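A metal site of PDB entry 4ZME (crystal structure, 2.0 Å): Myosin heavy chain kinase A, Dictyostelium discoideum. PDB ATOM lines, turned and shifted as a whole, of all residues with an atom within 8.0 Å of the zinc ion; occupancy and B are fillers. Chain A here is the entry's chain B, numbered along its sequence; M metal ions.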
ATOM      1  N   SER A 201     -14.085 -17.518 -13.201  1.00  0.00           N
ATOM      2  CA  SER A 201     -13.041 -16.829 -12.435  1.00  0.00           C
ATOM      3  C   SER A 201     -13.026 -15.314 -12.673  1.00  0.00           C
ATOM      4  O   SER A 201     -12.910 -14.533 -11.722  1.00  0.00           O
ATOM      5  CB  SER A 201     -11.670 -17.418 -12.784  1.00  0.00           C
ATOM      6  OG  SER A 201     -11.495 -18.687 -12.172  1.00  0.00           O
ATOM      7  N   GLN A 204     -15.279 -12.722 -10.707  1.00  0.00           N
ATOM      8  CA  GLN A 204     -14.942 -12.579  -9.289  1.00  0.00           C
ATOM      9  C   GLN A 204     -13.579 -11.899  -9.142  1.00  0.00           C
ATOM     10  O   GLN A 204     -13.382 -11.125  -8.178  1.00  0.00           O
ATOM     11  CB  GLN A 204     -14.954 -13.941  -8.572  1.00  0.00           C
ATOM     12  CG  GLN A 204     -16.192 -14.778  -8.852  1.00  0.00           C
ATOM     13  CD  GLN A 204     -17.494 -14.109  -8.467  1.00  0.00           C
ATOM     14  OE1 GLN A 204     -17.559 -13.294  -7.548  1.00  0.00           O
ATOM     15  NE2 GLN A 204     -18.560 -14.475  -9.162  1.00  0.00           N
ATOM     16  N   ALA A 205     -12.656 -12.186 -10.052  1.00  0.00           N
ATOM     17  CA  ALA A 205     -11.340 -11.547 -10.030  1.00  0.00           C
ATOM     18  C   ALA A 205     -11.510 -10.015 -10.299  1.00  0.00           C
ATOM     19  O   ALA A 205     -10.836  -9.182  -9.716  1.00  0.00           O
ATOM     20  CB  ALA A 205     -10.434 -12.160 -11.054  1.00  0.00           C
ATOM     21  N   PHE A 206     -12.428  -9.679 -11.189  1.00  0.00           N
ATOM     22  CA  PHE A 206     -12.684  -8.283 -11.491  1.00  0.00           C
ATOM     23  C   PHE A 206     -13.216  -7.582 -10.255  1.00  0.00           C
ATOM     24  O   PHE A 206     -12.737  -6.517  -9.911  1.00  0.00           O
ATOM     25  CB  PHE A 206     -13.619  -8.126 -12.678  1.00  0.00           C
ATOM     26  CG  PHE A 206     -14.069  -6.699 -12.876  1.00  0.00           C
ATOM     27  CD1 PHE A 206     -13.191  -5.781 -13.396  1.00  0.00           C
ATOM     28  CD2 PHE A 206     -15.307  -6.278 -12.449  1.00  0.00           C
ATOM     29  CE1 PHE A 206     -13.571  -4.457 -13.556  1.00  0.00           C
ATOM     30  CE2 PHE A 206     -15.697  -4.953 -12.618  1.00  0.00           C
ATOM     31  CZ  PHE A 206     -14.822  -4.048 -13.159  1.00  0.00           C
ATOM     32  N   SER A 207     -14.197  -8.168  -9.575  1.00  0.00           N
ATOM     33  CA  SER A 207     -14.731  -7.549  -8.344  1.00  0.00           C
ATOM     34  C   SER A 207     -13.615  -7.323  -7.313  1.00  0.00           C
ATOM     35  O   SER A 207     -13.507  -6.231  -6.742  1.00  0.00           O
ATOM     36  CB  SER A 207     -15.874  -8.360  -7.726  1.00  0.00           C
ATOM     37  OG  SER A 207     -17.013  -8.329  -8.569  1.00  0.00           O
ATOM     38  N   HIS A 208     -12.766  -8.335  -7.121  1.00  0.00           N
ATOM     39  CA  HIS A 208     -11.631  -8.239  -6.193  1.00  0.00           C
ATOM     40  C   HIS A 208     -10.651  -7.136  -6.628  1.00  0.00           C
ATOM     41  O   HIS A 208     -10.224  -6.344  -5.817  1.00  0.00           O
ATOM     42  CB  HIS A 208     -10.905  -9.601  -6.055  1.00  0.00           C
ATOM     43  CG  HIS A 208      -9.836  -9.641  -5.005  1.00  0.00           C
ATOM     44  ND1 HIS A 208      -9.015 -10.732  -4.821  1.00  0.00           N
ATOM     45  CD2 HIS A 208      -9.455  -8.736  -4.072  1.00  0.00           C
ATOM     46  CE1 HIS A 208      -8.169 -10.494  -3.841  1.00  0.00           C
ATOM     47  NE2 HIS A 208      -8.412  -9.288  -3.366  1.00  0.00           N
ATOM     48  N   PHE A 209     -10.318  -7.115  -7.927  1.00  0.00           N
ATOM     49  CA  PHE A 209      -9.456  -6.107  -8.519  1.00  0.00           C
ATOM     50  C   PHE A 209      -9.956  -4.701  -8.181  1.00  0.00           C
ATOM     51  O   PHE A 209      -9.170  -3.861  -7.754  1.00  0.00           O
ATOM     52  CB  PHE A 209      -9.398  -6.307 -10.020  1.00  0.00           C
ATOM     53  CG  PHE A 209      -8.578  -5.274 -10.780  1.00  0.00           C
ATOM     54  CD1 PHE A 209      -7.217  -5.427 -10.962  1.00  0.00           C
ATOM     55  CD2 PHE A 209      -9.209  -4.193 -11.395  1.00  0.00           C
ATOM     56  CE1 PHE A 209      -6.480  -4.486 -11.666  1.00  0.00           C
ATOM     57  CE2 PHE A 209      -8.472  -3.267 -12.133  1.00  0.00           C
ATOM     58  CZ  PHE A 209      -7.111  -3.409 -12.259  1.00  0.00           C
ATOM     59  N   GLU A 212      -9.290  -3.942  -4.396  1.00  0.00           N
ATOM     60  CA  GLU A 212      -7.921  -3.750  -3.985  1.00  0.00           C
ATOM     61  C   GLU A 212      -7.345  -2.475  -4.626  1.00  0.00           C
ATOM     62  O   GLU A 212      -6.797  -1.633  -3.933  1.00  0.00           O
ATOM     63  CB  GLU A 212      -7.057  -4.938  -4.352  1.00  0.00           C
ATOM     64  CG  GLU A 212      -5.624  -4.702  -3.879  1.00  0.00           C
ATOM     65  CD  GLU A 212      -4.756  -5.939  -3.900  1.00  0.00           C
ATOM     66  OE1 GLU A 212      -3.594  -5.802  -4.344  1.00  0.00           O
ATOM     67  OE2 GLU A 212      -5.219  -7.019  -3.476  1.00  0.00           O
ATOM     68  N   PHE A 256     -19.117  -9.310   0.421  1.00  0.00           N
ATOM     69  CA  PHE A 256     -18.326  -9.808  -0.707  1.00  0.00           C
ATOM     70  C   PHE A 256     -17.059 -10.540  -0.246  1.00  0.00           C
ATOM     71  O   PHE A 256     -16.687 -11.587  -0.793  1.00  0.00           O
ATOM     72  CB  PHE A 256     -17.915  -8.684  -1.664  1.00  0.00           C
ATOM     73  CG  PHE A 256     -16.973  -9.138  -2.737  1.00  0.00           C
ATOM     74  CD1 PHE A 256     -17.449  -9.748  -3.881  1.00  0.00           C
ATOM     75  CD2 PHE A 256     -15.605  -9.056  -2.558  1.00  0.00           C
ATOM     76  CE1 PHE A 256     -16.585 -10.243  -4.853  1.00  0.00           C
ATOM     77  CE2 PHE A 256     -14.733  -9.523  -3.526  1.00  0.00           C
ATOM     78  CZ  PHE A 256     -15.215 -10.120  -4.672  1.00  0.00           C
ATOM     79  N   HIS A 260     -15.770 -14.459  -0.853  1.00  0.00           N
ATOM     80  CA  HIS A 260     -14.809 -14.472  -1.958  1.00  0.00           C
ATOM     81  C   HIS A 260     -13.685 -15.461  -1.718  1.00  0.00           C
ATOM     82  O   HIS A 260     -13.040 -15.437  -0.685  1.00  0.00           O
ATOM     83  CB  HIS A 260     -14.212 -13.082  -2.235  1.00  0.00           C
ATOM     84  CG  HIS A 260     -13.220 -13.066  -3.353  1.00  0.00           C
ATOM     85  ND1 HIS A 260     -13.563 -13.239  -4.667  1.00  0.00           N
ATOM     86  CD2 HIS A 260     -11.869 -12.921  -3.336  1.00  0.00           C
ATOM     87  CE1 HIS A 260     -12.480 -13.203  -5.428  1.00  0.00           C
ATOM     88  NE2 HIS A 260     -11.440 -13.004  -4.629  1.00  0.00           N
ATOM     89  N   LYS A 261     -13.433 -16.297  -2.721  1.00  0.00           N
ATOM     90  CA  LYS A 261     -12.318 -17.206  -2.694  1.00  0.00           C
ATOM     91  C   LYS A 261     -11.492 -16.926  -3.929  1.00  0.00           C
ATOM     92  O   LYS A 261     -11.977 -17.032  -5.043  1.00  0.00           O
ATOM     93  CB  LYS A 261     -12.790 -18.661  -2.686  1.00  0.00           C
ATOM     94  CG  LYS A 261     -11.672 -19.626  -2.392  1.00  0.00           C
ATOM     95  CD  LYS A 261     -11.937 -21.005  -2.981  1.00  0.00           C
ATOM     96  CE  LYS A 261     -12.930 -21.776  -2.129  1.00  0.00           C
ATOM     97  NZ  LYS A 261     -12.645 -23.235  -2.292  1.00  0.00           N
ATOM     98  N   CYS A 262     -10.226 -16.536  -3.717  1.00  0.00           N
ATOM     99  CA  CYS A 262      -9.396 -16.109  -4.818  1.00  0.00           C
ATOM    100  C   CYS A 262      -9.221 -17.277  -5.740  1.00  0.00           C
ATOM    101  O   CYS A 262      -9.300 -18.432  -5.298  1.00  0.00           O
ATOM    102  CB  CYS A 262      -8.042 -15.580  -4.366  1.00  0.00           C
ATOM    103  SG  CYS A 262      -8.019 -13.873  -3.783  1.00  0.00           S
ATOM    104  N   ASN A 263      -8.998 -16.952  -7.008  1.00  0.00           N
ATOM    105  CA  ASN A 263      -8.796 -17.899  -8.084  1.00  0.00           C
ATOM    106  C   ASN A 263      -7.525 -17.568  -8.816  1.00  0.00           C
ATOM    107  O   ASN A 263      -6.777 -16.698  -8.385  1.00  0.00           O
ATOM    108  CB  ASN A 263      -9.996 -17.881  -9.043  1.00  0.00           C
ATOM    109  CG  ASN A 263     -10.292 -16.493  -9.609  1.00  0.00           C
ATOM    110  OD1 ASN A 263      -9.493 -15.918 -10.336  1.00  0.00           O
ATOM    111  ND2 ASN A 263     -11.479 -15.969  -9.310  1.00  0.00           N
ATOM    112  N   ALA A 264      -7.249 -18.254  -9.921  1.00  0.00           N
ATOM    113  CA  ALA A 264      -6.031 -18.032 -10.712  1.00  0.00           C
ATOM    114  C   ALA A 264      -5.899 -16.658 -11.340  1.00  0.00           C
ATOM    115  O   ALA A 264      -4.777 -16.173 -11.545  1.00  0.00           O
ATOM    116  CB  ALA A 264      -5.956 -19.055 -11.820  1.00  0.00           C
ATOM    117  N   VAL A 265      -7.022 -16.029 -11.708  1.00  0.00           N
ATOM    118  CA  VAL A 265      -6.944 -14.688 -12.296  1.00  0.00           C
ATOM    119  C   VAL A 265      -6.546 -13.688 -11.207  1.00  0.00           C
ATOM    120  O   VAL A 265      -5.769 -12.816 -11.477  1.00  0.00           O
ATOM    121  CB  VAL A 265      -8.239 -14.282 -13.001  1.00  0.00           C
ATOM    122  CG1 VAL A 265      -8.087 -12.900 -13.641  1.00  0.00           C
ATOM    123  CG2 VAL A 265      -8.607 -15.298 -14.084  1.00  0.00           C
ATOM    124  N   CYS A 266      -7.091 -13.829  -9.997  1.00  0.00           N
ATOM    125  CA  CYS A 266      -6.679 -13.029  -8.823  1.00  0.00           C
ATOM    126  C   CYS A 266      -5.152 -13.105  -8.664  1.00  0.00           C
ATOM    127  O   CYS A 266      -4.488 -12.103  -8.529  1.00  0.00           O
ATOM    128  CB  CYS A 266      -7.311 -13.486  -7.508  1.00  0.00           C
ATOM    129  SG  CYS A 266      -9.060 -13.224  -7.125  1.00  0.00           S
ATOM    130  N   ALA A 267      -4.614 -14.309  -8.682  1.00  0.00           N
ATOM    131  CA  ALA A 267      -3.162 -14.523  -8.547  1.00  0.00           C
ATOM    132  C   ALA A 267      -2.409 -13.887  -9.700  1.00  0.00           C
ATOM    133  O   ALA A 267      -1.405 -13.219  -9.499  1.00  0.00           O
ATOM    134  CB  ALA A 267      -2.857 -16.020  -8.471  1.00  0.00           C
ATOM    135  N   LEU A 269      -3.208 -11.365 -11.474  1.00  0.00           N
ATOM    136  CA  LEU A 269      -3.251  -9.903 -11.281  1.00  0.00           C
ATOM    137  C   LEU A 269      -2.517  -9.448 -10.021  1.00  0.00           C
ATOM    138  O   LEU A 269      -2.585  -8.282  -9.652  1.00  0.00           O
ATOM    139  CB  LEU A 269      -4.706  -9.460 -11.179  1.00  0.00           C
ATOM    140  CG  LEU A 269      -5.489  -9.609 -12.471  1.00  0.00           C
ATOM    141  CD1 LEU A 269      -6.978  -9.582 -12.170  1.00  0.00           C
ATOM    142  CD2 LEU A 269      -5.101  -8.506 -13.436  1.00  0.00           C
ATOM    143  N   LEU A 271      -3.140  -9.938  -6.898  1.00  0.00           N
ATOM    144  CA  LEU A 271      -3.994  -9.505  -5.822  1.00  0.00           C
ATOM    145  C   LEU A 271      -3.710 -10.280  -4.557  1.00  0.00           C
ATOM    146  O   LEU A 271      -3.364 -11.459  -4.586  1.00  0.00           O
ATOM    147  CB  LEU A 271      -5.464  -9.703  -6.212  1.00  0.00           C
ATOM    148  CG  LEU A 271      -5.903  -9.036  -7.524  1.00  0.00           C
ATOM    149  CD1 LEU A 271      -7.388  -9.256  -7.754  1.00  0.00           C
ATOM    150  CD2 LEU A 271      -5.597  -7.544  -7.505  1.00  0.00           C
ATOM    151  N   ASP A 272      -3.873  -9.600  -3.434  1.00  0.00           N
ATOM    152  CA  ASP A 272      -3.691 -10.182  -2.115  1.00  0.00           C
ATOM    153  C   ASP A 272      -4.626 -11.383  -1.878  1.00  0.00           C
ATOM    154  O   ASP A 272      -5.854 -11.240  -1.869  1.00  0.00           O
ATOM    155  CB  ASP A 272      -3.942  -9.084  -1.087  1.00  0.00           C
ATOM    156  CG  ASP A 272      -3.316  -9.369   0.249  1.00  0.00           C
ATOM    157  OD1 ASP A 272      -3.445 -10.503   0.753  1.00  0.00           O
ATOM    158  OD2 ASP A 272      -2.711  -8.415   0.806  1.00  0.00           O
ATOM    159  N   VAL A 273      -4.033 -12.562  -1.660  1.00  0.00           N
ATOM    160  CA  VAL A 273      -4.774 -13.841  -1.643  1.00  0.00           C
ATOM    161  C   VAL A 273      -5.811 -13.898  -0.541  1.00  0.00           C
ATOM    162  O   VAL A 273      -6.742 -14.691  -0.621  1.00  0.00           O
ATOM    163  CB  VAL A 273      -3.836 -15.079  -1.559  1.00  0.00           C
ATOM    164  CG1 VAL A 273      -4.639 -16.359  -1.357  1.00  0.00           C
ATOM    165  CG2 VAL A 273      -2.980 -15.194  -2.804  1.00  0.00           C
ATOM    166  N   LYS A 274      -5.632 -13.078   0.494  1.00  0.00           N
ATOM    167  CA  LYS A 274      -6.768 -12.664   1.319  1.00  0.00           C
ATOM    168  C   LYS A 274      -6.924 -11.128   1.477  1.00  0.00           C
ATOM    169  O   LYS A 274      -5.962 -10.379   1.582  1.00  0.00           O
ATOM    170  CB  LYS A 274      -6.724 -13.359   2.682  1.00  0.00           C
ATOM    171  CG  LYS A 274      -8.082 -13.374   3.376  1.00  0.00           C
ATOM    172  CD  LYS A 274      -8.020 -13.786   4.836  1.00  0.00           C
ATOM    173  CE  LYS A 274      -8.957 -12.917   5.656  1.00  0.00           C
ATOM    174  NZ  LYS A 274      -9.174 -13.384   7.037  1.00  0.00           N
ATOM    175  N   LEU A 275      -8.178 -10.694   1.525  1.00  0.00           N
ATOM    176  CA  LEU A 275      -8.545  -9.275   1.449  1.00  0.00           C
ATOM    177  C   LEU A 275      -8.504  -8.521   2.767  1.00  0.00           C
ATOM    178  O   LEU A 275      -8.743  -9.111   3.828  1.00  0.00           O
ATOM    179  CB  LEU A 275      -9.993  -9.139   0.956  1.00  0.00           C
ATOM    180  CG  LEU A 275     -10.217  -9.407  -0.522  1.00  0.00           C
ATOM    181  CD1 LEU A 275      -9.953 -10.861  -0.847  1.00  0.00           C
ATOM    182  CD2 LEU A 275     -11.617  -9.025  -0.938  1.00  0.00           C
HETATM  183 ZN    ZN M   1      -9.481 -12.753  -5.346  1.00  0.00          ZN
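Of the 23 residues printed, 4 come within 4 Å of the zinc ion.
The zinc ion is bound by the side-chain sulfur of Cys 266, a ring nitrogen (NE2) of His 260, a ring nitrogen (ND1) of His 208 and the side-chain sulfur of Cys 262. The zinc ion has four donor atoms within binding distance.
The backbone NH of Cys 266 sits at hydrogen-bond distance from the side-chain amide oxygen of Asn 263 (3.2 Å). The backbone carbonyl oxygen (O) of Cys 266 is in hydrogen-bond range of the backbone NH (N) of Leu 271, 3.0 Å away. SG of Cys 262 sits close to O of Val 273, 3.5 Å away.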
